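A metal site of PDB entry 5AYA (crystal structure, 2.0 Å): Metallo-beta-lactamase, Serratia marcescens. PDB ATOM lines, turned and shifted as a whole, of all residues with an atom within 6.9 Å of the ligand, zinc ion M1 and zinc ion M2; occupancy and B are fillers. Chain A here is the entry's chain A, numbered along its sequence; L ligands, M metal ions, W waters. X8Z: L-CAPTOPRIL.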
ATOM      1  N   TRP A   5      23.424 -11.596  22.219  1.00  0.00           N
ATOM      2  CA  TRP A   5      22.811 -12.618  21.399  1.00  0.00           C
ATOM      3  C   TRP A   5      21.272 -12.608  21.509  1.00  0.00           C
ATOM      4  O   TRP A   5      20.586 -13.135  20.627  1.00  0.00           O
ATOM      5  CB  TRP A   5      23.344 -14.012  21.791  1.00  0.00           C
ATOM      6  CG  TRP A   5      24.844 -14.195  21.593  1.00  0.00           C
ATOM      7  CD1 TRP A   5      25.694 -13.406  20.846  1.00  0.00           C
ATOM      8  CD2 TRP A   5      25.649 -15.276  22.100  1.00  0.00           C
ATOM      9  NE1 TRP A   5      26.971 -13.927  20.871  1.00  0.00           N
ATOM     10  CE2 TRP A   5      26.975 -15.075  21.625  1.00  0.00           C
ATOM     11  CE3 TRP A   5      25.384 -16.391  22.905  1.00  0.00           C
ATOM     12  CZ2 TRP A   5      28.021 -15.943  21.932  1.00  0.00           C
ATOM     13  CZ3 TRP A   5      26.440 -17.258  23.221  1.00  0.00           C
ATOM     14  CH2 TRP A   5      27.749 -17.009  22.747  1.00  0.00           C
ATOM     15  N   ILE A  26      23.024 -12.193  16.671  1.00  0.00           N
ATOM     16  CA  ILE A  26      22.904 -13.458  15.926  1.00  0.00           C
ATOM     17  C   ILE A  26      21.925 -13.314  14.766  1.00  0.00           C
ATOM     18  O   ILE A  26      20.833 -12.810  14.956  1.00  0.00           O
ATOM     19  CB  ILE A  26      22.389 -14.593  16.837  1.00  0.00           C
ATOM     20  CG1 ILE A  26      23.334 -14.817  18.019  1.00  0.00           C
ATOM     21  CG2 ILE A  26      22.218 -15.894  16.049  1.00  0.00           C
ATOM     22  CD1 ILE A  26      24.603 -15.556  17.659  1.00  0.00           C
ATOM     23  N   HIS A  72      23.302 -24.764  12.935  1.00  0.00           N
ATOM     24  CA  HIS A  72      23.783 -25.770  13.901  1.00  0.00           C
ATOM     25  C   HIS A  72      23.275 -25.589  15.337  1.00  0.00           C
ATOM     26  O   HIS A  72      22.793 -24.503  15.715  1.00  0.00           O
ATOM     27  CB  HIS A  72      25.305 -25.797  13.892  1.00  0.00           C
ATOM     28  CG  HIS A  72      25.930 -24.627  14.558  1.00  0.00           C
ATOM     29  ND1 HIS A  72      26.307 -23.485  13.869  1.00  0.00           N
ATOM     30  CD2 HIS A  72      26.230 -24.399  15.854  1.00  0.00           C
ATOM     31  CE1 HIS A  72      26.762 -22.592  14.726  1.00  0.00           C
ATOM     32  NE2 HIS A  72      26.751 -23.136  15.933  1.00  0.00           N
ATOM     33  N   SER A  73      23.516 -26.608  16.158  1.00  0.00           N
ATOM     34  CA  SER A  73      22.735 -26.832  17.388  1.00  0.00           C
ATOM     35  C   SER A  73      23.499 -26.388  18.617  1.00  0.00           C
ATOM     36  O   SER A  73      23.668 -27.150  19.567  1.00  0.00           O
ATOM     37  CB  SER A  73      22.376 -28.321  17.515  1.00  0.00           C
ATOM     38  OG  SER A  73      23.506 -29.144  17.285  1.00  0.00           O
ATOM     39  N   HIS A  74      24.052 -25.179  18.566  1.00  0.00           N
ATOM     40  CA  HIS A  74      24.471 -24.489  19.763  1.00  0.00           C
ATOM     41  C   HIS A  74      23.404 -23.512  20.191  1.00  0.00           C
ATOM     42  O   HIS A  74      22.651 -23.011  19.340  1.00  0.00           O
ATOM     43  CB  HIS A  74      25.756 -23.736  19.525  1.00  0.00           C
ATOM     44  CG  HIS A  74      26.926 -24.630  19.339  1.00  0.00           C
ATOM     45  ND1 HIS A  74      28.149 -24.172  18.928  1.00  0.00           N
ATOM     46  CD2 HIS A  74      27.067 -25.955  19.555  1.00  0.00           C
ATOM     47  CE1 HIS A  74      28.988 -25.187  18.843  1.00  0.00           C
ATOM     48  NE2 HIS A  74      28.365 -26.282  19.227  1.00  0.00           N
ATOM     49  N   GLU A  75      23.358 -23.255  21.489  1.00  0.00           N
ATOM     50  CA  GLU A  75      22.278 -22.514  22.146  1.00  0.00           C
ATOM     51  C   GLU A  75      21.965 -21.156  21.493  1.00  0.00           C
ATOM     52  O   GLU A  75      20.792 -20.792  21.303  1.00  0.00           O
ATOM     53  CB  GLU A  75      22.611 -22.341  23.637  1.00  0.00           C
ATOM     54  CG  GLU A  75      23.898 -21.555  23.906  1.00  0.00           C
ATOM     55  CD  GLU A  75      24.286 -21.498  25.387  1.00  0.00           C
ATOM     56  OE1 GLU A  75      23.427 -21.796  26.254  1.00  0.00           O
ATOM     57  OE2 GLU A  75      25.446 -21.108  25.685  1.00  0.00           O
ATOM     58  N   ASP A  76      23.015 -20.452  21.101  1.00  0.00           N
ATOM     59  CA  ASP A  76      22.906 -19.109  20.562  1.00  0.00           C
ATOM     60  C   ASP A  76      22.215 -19.006  19.172  1.00  0.00           C
ATOM     61  O   ASP A  76      21.765 -17.908  18.814  1.00  0.00           O
ATOM     62  CB  ASP A  76      24.272 -18.390  20.545  1.00  0.00           C
ATOM     63  CG  ASP A  76      25.326 -19.103  19.712  1.00  0.00           C
ATOM     64  OD1 ASP A  76      25.290 -20.360  19.604  1.00  0.00           O
ATOM     65  OD2 ASP A  76      26.260 -18.414  19.263  1.00  0.00           O
ATOM     66  N   HIS A  77      22.107 -20.119  18.439  1.00  0.00           N
ATOM     67  CA  HIS A  77      21.353 -20.151  17.163  1.00  0.00           C
ATOM     68  C   HIS A  77      20.076 -20.947  17.277  1.00  0.00           C
ATOM     69  O   HIS A  77      19.128 -20.702  16.533  1.00  0.00           O
ATOM     70  CB  HIS A  77      22.197 -20.790  16.056  1.00  0.00           C
ATOM     71  CG  HIS A  77      23.568 -20.225  15.963  1.00  0.00           C
ATOM     72  ND1 HIS A  77      23.822 -18.970  15.448  1.00  0.00           N
ATOM     73  CD2 HIS A  77      24.755 -20.683  16.446  1.00  0.00           C
ATOM     74  CE1 HIS A  77      25.114 -18.708  15.541  1.00  0.00           C
ATOM     75  NE2 HIS A  77      25.682 -19.696  16.217  1.00  0.00           N
ATOM     76  N   ASP A 111      30.304 -33.127  20.319  1.00  0.00           N
ATOM     77  CA  ASP A 111      30.317 -31.689  20.050  1.00  0.00           C
ATOM     78  C   ASP A 111      31.533 -31.021  20.710  1.00  0.00           C
ATOM     79  O   ASP A 111      31.839 -31.256  21.886  1.00  0.00           O
ATOM     80  CB  ASP A 111      29.026 -31.051  20.558  1.00  0.00           C
ATOM     81  CG  ASP A 111      28.713 -29.724  19.865  1.00  0.00           C
ATOM     82  OD1 ASP A 111      28.098 -29.758  18.780  1.00  0.00           O
ATOM     83  OD2 ASP A 111      29.109 -28.660  20.380  1.00  0.00           O
ATOM     84  N   GLN A 113      31.769 -28.187  21.855  1.00  0.00           N
ATOM     85  CA  GLN A 113      31.311 -27.352  22.971  1.00  0.00           C
ATOM     86  C   GLN A 113      30.306 -28.054  23.879  1.00  0.00           C
ATOM     87  O   GLN A 113      29.612 -27.400  24.656  1.00  0.00           O
ATOM     88  CB  GLN A 113      30.717 -26.052  22.436  1.00  0.00           C
ATOM     89  CG  GLN A 113      31.726 -25.219  21.664  1.00  0.00           C
ATOM     90  CD  GLN A 113      31.186 -23.861  21.277  1.00  0.00           C
ATOM     91  OE1 GLN A 113      30.292 -23.329  21.927  1.00  0.00           O
ATOM     92  NE2 GLN A 113      31.674 -23.325  20.176  1.00  0.00           N
ATOM     93  N   LEU A 117      29.076 -25.078  26.412  1.00  0.00           N
ATOM     94  CA  LEU A 117      27.716 -24.586  26.189  1.00  0.00           C
ATOM     95  C   LEU A 117      26.708 -25.395  26.988  1.00  0.00           C
ATOM     96  O   LEU A 117      26.437 -26.562  26.677  1.00  0.00           O
ATOM     97  CB  LEU A 117      27.341 -24.649  24.705  1.00  0.00           C
ATOM     98  CG  LEU A 117      28.085 -23.714  23.744  1.00  0.00           C
ATOM     99  CD1 LEU A 117      27.169 -23.305  22.616  1.00  0.00           C
ATOM    100  CD2 LEU A 117      28.641 -22.471  24.445  1.00  0.00           C
ATOM    101  N   HIS A 150      32.334 -27.631  12.936  1.00  0.00           N
ATOM    102  CA  HIS A 150      32.040 -26.859  14.133  1.00  0.00           C
ATOM    103  C   HIS A 150      31.020 -27.662  14.935  1.00  0.00           C
ATOM    104  O   HIS A 150      31.025 -27.632  16.168  1.00  0.00           O
ATOM    105  CB  HIS A 150      31.502 -25.452  13.723  1.00  0.00           C
ATOM    106  CG  HIS A 150      31.100 -24.559  14.860  1.00  0.00           C
ATOM    107  ND1 HIS A 150      31.964 -23.630  15.393  1.00  0.00           N
ATOM    108  CD2 HIS A 150      29.895 -24.321  15.430  1.00  0.00           C
ATOM    109  CE1 HIS A 150      31.335 -22.924  16.315  1.00  0.00           C
ATOM    110  NE2 HIS A 150      30.077 -23.316  16.362  1.00  0.00           N
ATOM    111  N   THR A 151      30.090 -28.284  14.199  1.00  0.00           N
ATOM    112  CA  THR A 151      29.214 -29.332  14.714  1.00  0.00           C
ATOM    113  C   THR A 151      29.143 -30.400  13.625  1.00  0.00           C
ATOM    114  O   THR A 151      29.441 -30.109  12.454  1.00  0.00           O
ATOM    115  CB  THR A 151      27.771 -28.867  14.991  1.00  0.00           C
ATOM    116  OG1 THR A 151      27.146 -28.499  13.751  1.00  0.00           O
ATOM    117  CG2 THR A 151      27.725 -27.682  15.987  1.00  0.00           C
ATOM    118  N   ASP A 174      26.778 -21.199   7.752  1.00  0.00           N
ATOM    119  CA  ASP A 174      27.001 -21.775   9.072  1.00  0.00           C
ATOM    120  C   ASP A 174      28.387 -21.386   9.555  1.00  0.00           C
ATOM    121  O   ASP A 174      29.238 -21.006   8.761  1.00  0.00           O
ATOM    122  CB  ASP A 174      26.891 -23.294   9.014  1.00  0.00           C
ATOM    123  CG  ASP A 174      26.633 -23.930  10.392  1.00  0.00           C
ATOM    124  OD1 ASP A 174      26.312 -23.183  11.347  1.00  0.00           O
ATOM    125  OD2 ASP A 174      26.843 -25.140  10.525  1.00  0.00           O
ATOM    126  N   SER A 175      28.603 -21.478  10.881  1.00  0.00           N
ATOM    127  CA  SER A 175      29.926 -21.210  11.452  1.00  0.00           C
ATOM    128  C   SER A 175      30.899 -22.283  11.023  1.00  0.00           C
ATOM    129  O   SER A 175      30.596 -23.487  11.072  1.00  0.00           O
ATOM    130  CB  SER A 175      29.882 -21.130  12.994  1.00  0.00           C
ATOM    131  OG  SER A 175      28.753 -20.387  13.430  1.00  0.00           O
ATOM    132  N   LEU A 176      32.099 -21.846  10.657  1.00  0.00           N
ATOM    133  CA  LEU A 176      33.194 -22.720  10.242  1.00  0.00           C
ATOM    134  C   LEU A 176      34.390 -22.605  11.210  1.00  0.00           C
ATOM    135  O   LEU A 176      35.521 -22.986  10.861  1.00  0.00           O
ATOM    136  CB  LEU A 176      33.627 -22.338   8.834  1.00  0.00           C
ATOM    137  CG  LEU A 176      32.511 -22.367   7.752  1.00  0.00           C
ATOM    138  CD1 LEU A 176      33.053 -21.818   6.437  1.00  0.00           C
ATOM    139  CD2 LEU A 176      31.978 -23.780   7.583  1.00  0.00           C
ATOM    140  N   THR A 177      34.103 -22.235  12.443  1.00  0.00           N
ATOM    141  CA  THR A 177      35.125 -21.929  13.441  1.00  0.00           C
ATOM    142  C   THR A 177      35.497 -23.154  14.288  1.00  0.00           C
ATOM    143  O   THR A 177      34.622 -23.851  14.836  1.00  0.00           O
ATOM    144  CB  THR A 177      34.696 -20.748  14.343  1.00  0.00           C
ATOM    145  OG1 THR A 177      33.343 -20.896  14.796  1.00  0.00           O
ATOM    146  CG2 THR A 177      34.828 -19.444  13.574  1.00  0.00           C
ATOM    147  N   VAL A 179      36.274 -24.012  17.412  1.00  0.00           N
ATOM    148  CA  VAL A 179      36.229 -23.614  18.805  1.00  0.00           C
ATOM    149  C   VAL A 179      35.483 -24.676  19.568  1.00  0.00           C
ATOM    150  O   VAL A 179      34.707 -25.421  18.994  1.00  0.00           O
ATOM    151  CB  VAL A 179      35.532 -22.257  19.000  1.00  0.00           C
ATOM    152  CG1 VAL A 179      36.441 -21.122  18.553  1.00  0.00           C
ATOM    153  CG2 VAL A 179      34.210 -22.207  18.256  1.00  0.00           C
ATOM    154  N   ALA A 214      26.067 -16.655  10.240  1.00  0.00           N
ATOM    155  CA  ALA A 214      25.270 -16.931  11.443  1.00  0.00           C
ATOM    156  C   ALA A 214      25.590 -15.889  12.515  1.00  0.00           C
ATOM    157  O   ALA A 214      24.686 -15.283  13.106  1.00  0.00           O
ATOM    158  CB  ALA A 214      25.564 -18.343  11.950  1.00  0.00           C
ATOM    159  N   HIS A 215      26.884 -15.662  12.725  1.00  0.00           N
ATOM    160  CA  HIS A 215      27.351 -14.431  13.380  1.00  0.00           C
ATOM    161  C   HIS A 215      27.536 -13.295  12.354  1.00  0.00           C
ATOM    162  O   HIS A 215      28.485 -13.282  11.566  1.00  0.00           O
ATOM    163  CB  HIS A 215      28.649 -14.701  14.164  1.00  0.00           C
ATOM    164  CG  HIS A 215      28.451 -15.570  15.379  1.00  0.00           C
ATOM    165  ND1 HIS A 215      27.929 -15.100  16.564  1.00  0.00           N
ATOM    166  CD2 HIS A 215      28.614 -16.904  15.536  1.00  0.00           C
ATOM    167  CE1 HIS A 215      27.788 -16.108  17.410  1.00  0.00           C
ATOM    168  NE2 HIS A 215      28.194 -17.215  16.814  1.00  0.00           N
ATOM    169  N   GLU A 217      28.429 -10.204  12.000  1.00  0.00           N
ATOM    170  CA  GLU A 217      29.642  -9.430  11.755  1.00  0.00           C
ATOM    171  C   GLU A 217      30.699 -10.177  10.937  1.00  0.00           C
ATOM    172  O   GLU A 217      31.551  -9.544  10.317  1.00  0.00           O
ATOM    173  CB  GLU A 217      30.237  -8.934  13.080  1.00  0.00           C
ATOM    174  CG  GLU A 217      31.033  -9.954  13.877  1.00  0.00           C
ATOM    175  CD  GLU A 217      30.160 -10.946  14.602  1.00  0.00           C
ATOM    176  OE1 GLU A 217      28.942 -10.695  14.735  1.00  0.00           O
ATOM    177  OE2 GLU A 217      30.693 -11.989  15.028  1.00  0.00           O
ATOM    178  N   VAL A 218      30.566 -11.496  10.813  1.00  0.00           N
ATOM    179  CA  VAL A 218      31.551 -12.287  10.090  1.00  0.00           C
ATOM    180  C   VAL A 218      31.530 -11.958   8.594  1.00  0.00           C
ATOM    181  O   VAL A 218      32.529 -12.197   7.894  1.00  0.00           O
ATOM    182  CB  VAL A 218      31.302 -13.811  10.280  1.00  0.00           C
ATOM    183  CG1 VAL A 218      32.237 -14.638   9.412  1.00  0.00           C
ATOM    184  CG2 VAL A 218      31.471 -14.205  11.754  1.00  0.00           C
ATOM    185  N   ARG A 252      41.615 -19.856  11.080  1.00  0.00           N
ATOM    186  CA  ARG A 252      41.269 -20.110  12.459  1.00  0.00           C
ATOM    187  C   ARG A 252      41.606 -21.544  12.884  1.00  0.00           C
ATOM    188  O   ARG A 252      41.984 -21.780  14.029  1.00  0.00           O
ATOM    189  CB  ARG A 252      39.780 -19.831  12.681  1.00  0.00           C
ATOM    190  CG  ARG A 252      39.333 -19.992  14.120  1.00  0.00           C
ATOM    191  CD  ARG A 252      39.973 -18.962  15.041  1.00  0.00           C
ATOM    192  NE  ARG A 252      39.115 -18.707  16.193  1.00  0.00           N
ATOM    193  CZ  ARG A 252      37.997 -17.985  16.159  1.00  0.00           C
ATOM    194  NH1 ARG A 252      37.643 -17.346  15.043  1.00  0.00           N
ATOM    195  NH2 ARG A 252      37.241 -17.873  17.249  1.00  0.00           N
HETATM  196  O1  X8Z L   1      31.949 -18.598  15.682  1.00  0.00           O
HETATM  197  C4  X8Z L   1      31.592 -18.049  16.720  1.00  0.00           C
HETATM  198  C2  X8Z L   1      30.800 -18.843  17.735  1.00  0.00           C
HETATM  199  C1  X8Z L   1      30.067 -19.929  16.983  1.00  0.00           C
HETATM  200  S   X8Z L   1      28.784 -20.684  17.971  1.00  0.00           S
HETATM  201  C3  X8Z L   1      31.675 -19.406  18.865  1.00  0.00           C
HETATM  202  N   X8Z L   1      31.792 -16.755  17.014  1.00  0.00           N
HETATM  203  C8  X8Z L   1      32.369 -15.824  16.033  1.00  0.00           C
HETATM  204  C9  X8Z L   1      33.753 -16.198  15.620  1.00  0.00           C
HETATM  205  O3  X8Z L   1      34.568 -16.717  16.534  1.00  0.00           O
HETATM  206  O2  X8Z L   1      34.148 -15.958  14.488  1.00  0.00           O
HETATM  207  C5  X8Z L   1      31.453 -16.090  18.276  1.00  0.00           C
HETATM  208  C6  X8Z L   1      31.793 -14.612  18.095  1.00  0.00           C
HETATM  209  C7  X8Z L   1      32.441 -14.468  16.729  1.00  0.00           C
HETATM  210 ZN    ZN M   1      27.122 -19.054  17.539  1.00  0.00          ZN
HETATM  211 ZN    ZN M   2      28.365 -22.799  17.325  1.00  0.00          ZN
HETATM  212  O   HOH W   1      31.670 -17.784  12.938  1.00  0.00           O
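The side-chain hydroxyl (OG1) of Thr 177 lies within hydrogen-bond range of an oxygen (O1) of the ligand, at 2.8 Å.
The guanidinium group (NH2) of Arg 252 is in salt-bridge range of an oxygen (O3) of the ligand, at 3.0 Å.
Merely in contact with the ligand: Glu 217 (3.5 Å), Ser 175 (3.8 Å) and Val 179 (3.8 Å).
Of the 23 residues printed, 11 come within 4 Å of the ligand.
Of the 23 residues printed, 3 come within 4 Å of zinc ion M1.
The nearest printed residue that does not touch zinc ion M1 is Ile 26 (4.3 Å).
Zinc ion M1 is bound by OD2 of Asp 76, NE2 of His 77, NE2 of His 215 and S of the ligand.
A ring nitrogen (NE2) of His 74 sits at hydrogen-bond distance from the side-chain carboxylate of Asp 111.
ND1 of His 72 sits at hydrogen-bond distance from OD1 of Asp 174 (2.5 Å).
The backbone carbonyl oxygen of Thr 177 lies within hydrogen-bond range of a ring nitrogen (ND1) of His 150.
Zinc ion M2 is bound by NE2 of His 150 (2.0 Å), ND1 of His 74 (2.1 Å), NE2 of His 72 (2.2 Å) and S of the ligand (2.3 Å).
Of the 23 residues printed, 3 come within 4 Å of zinc ion M2.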
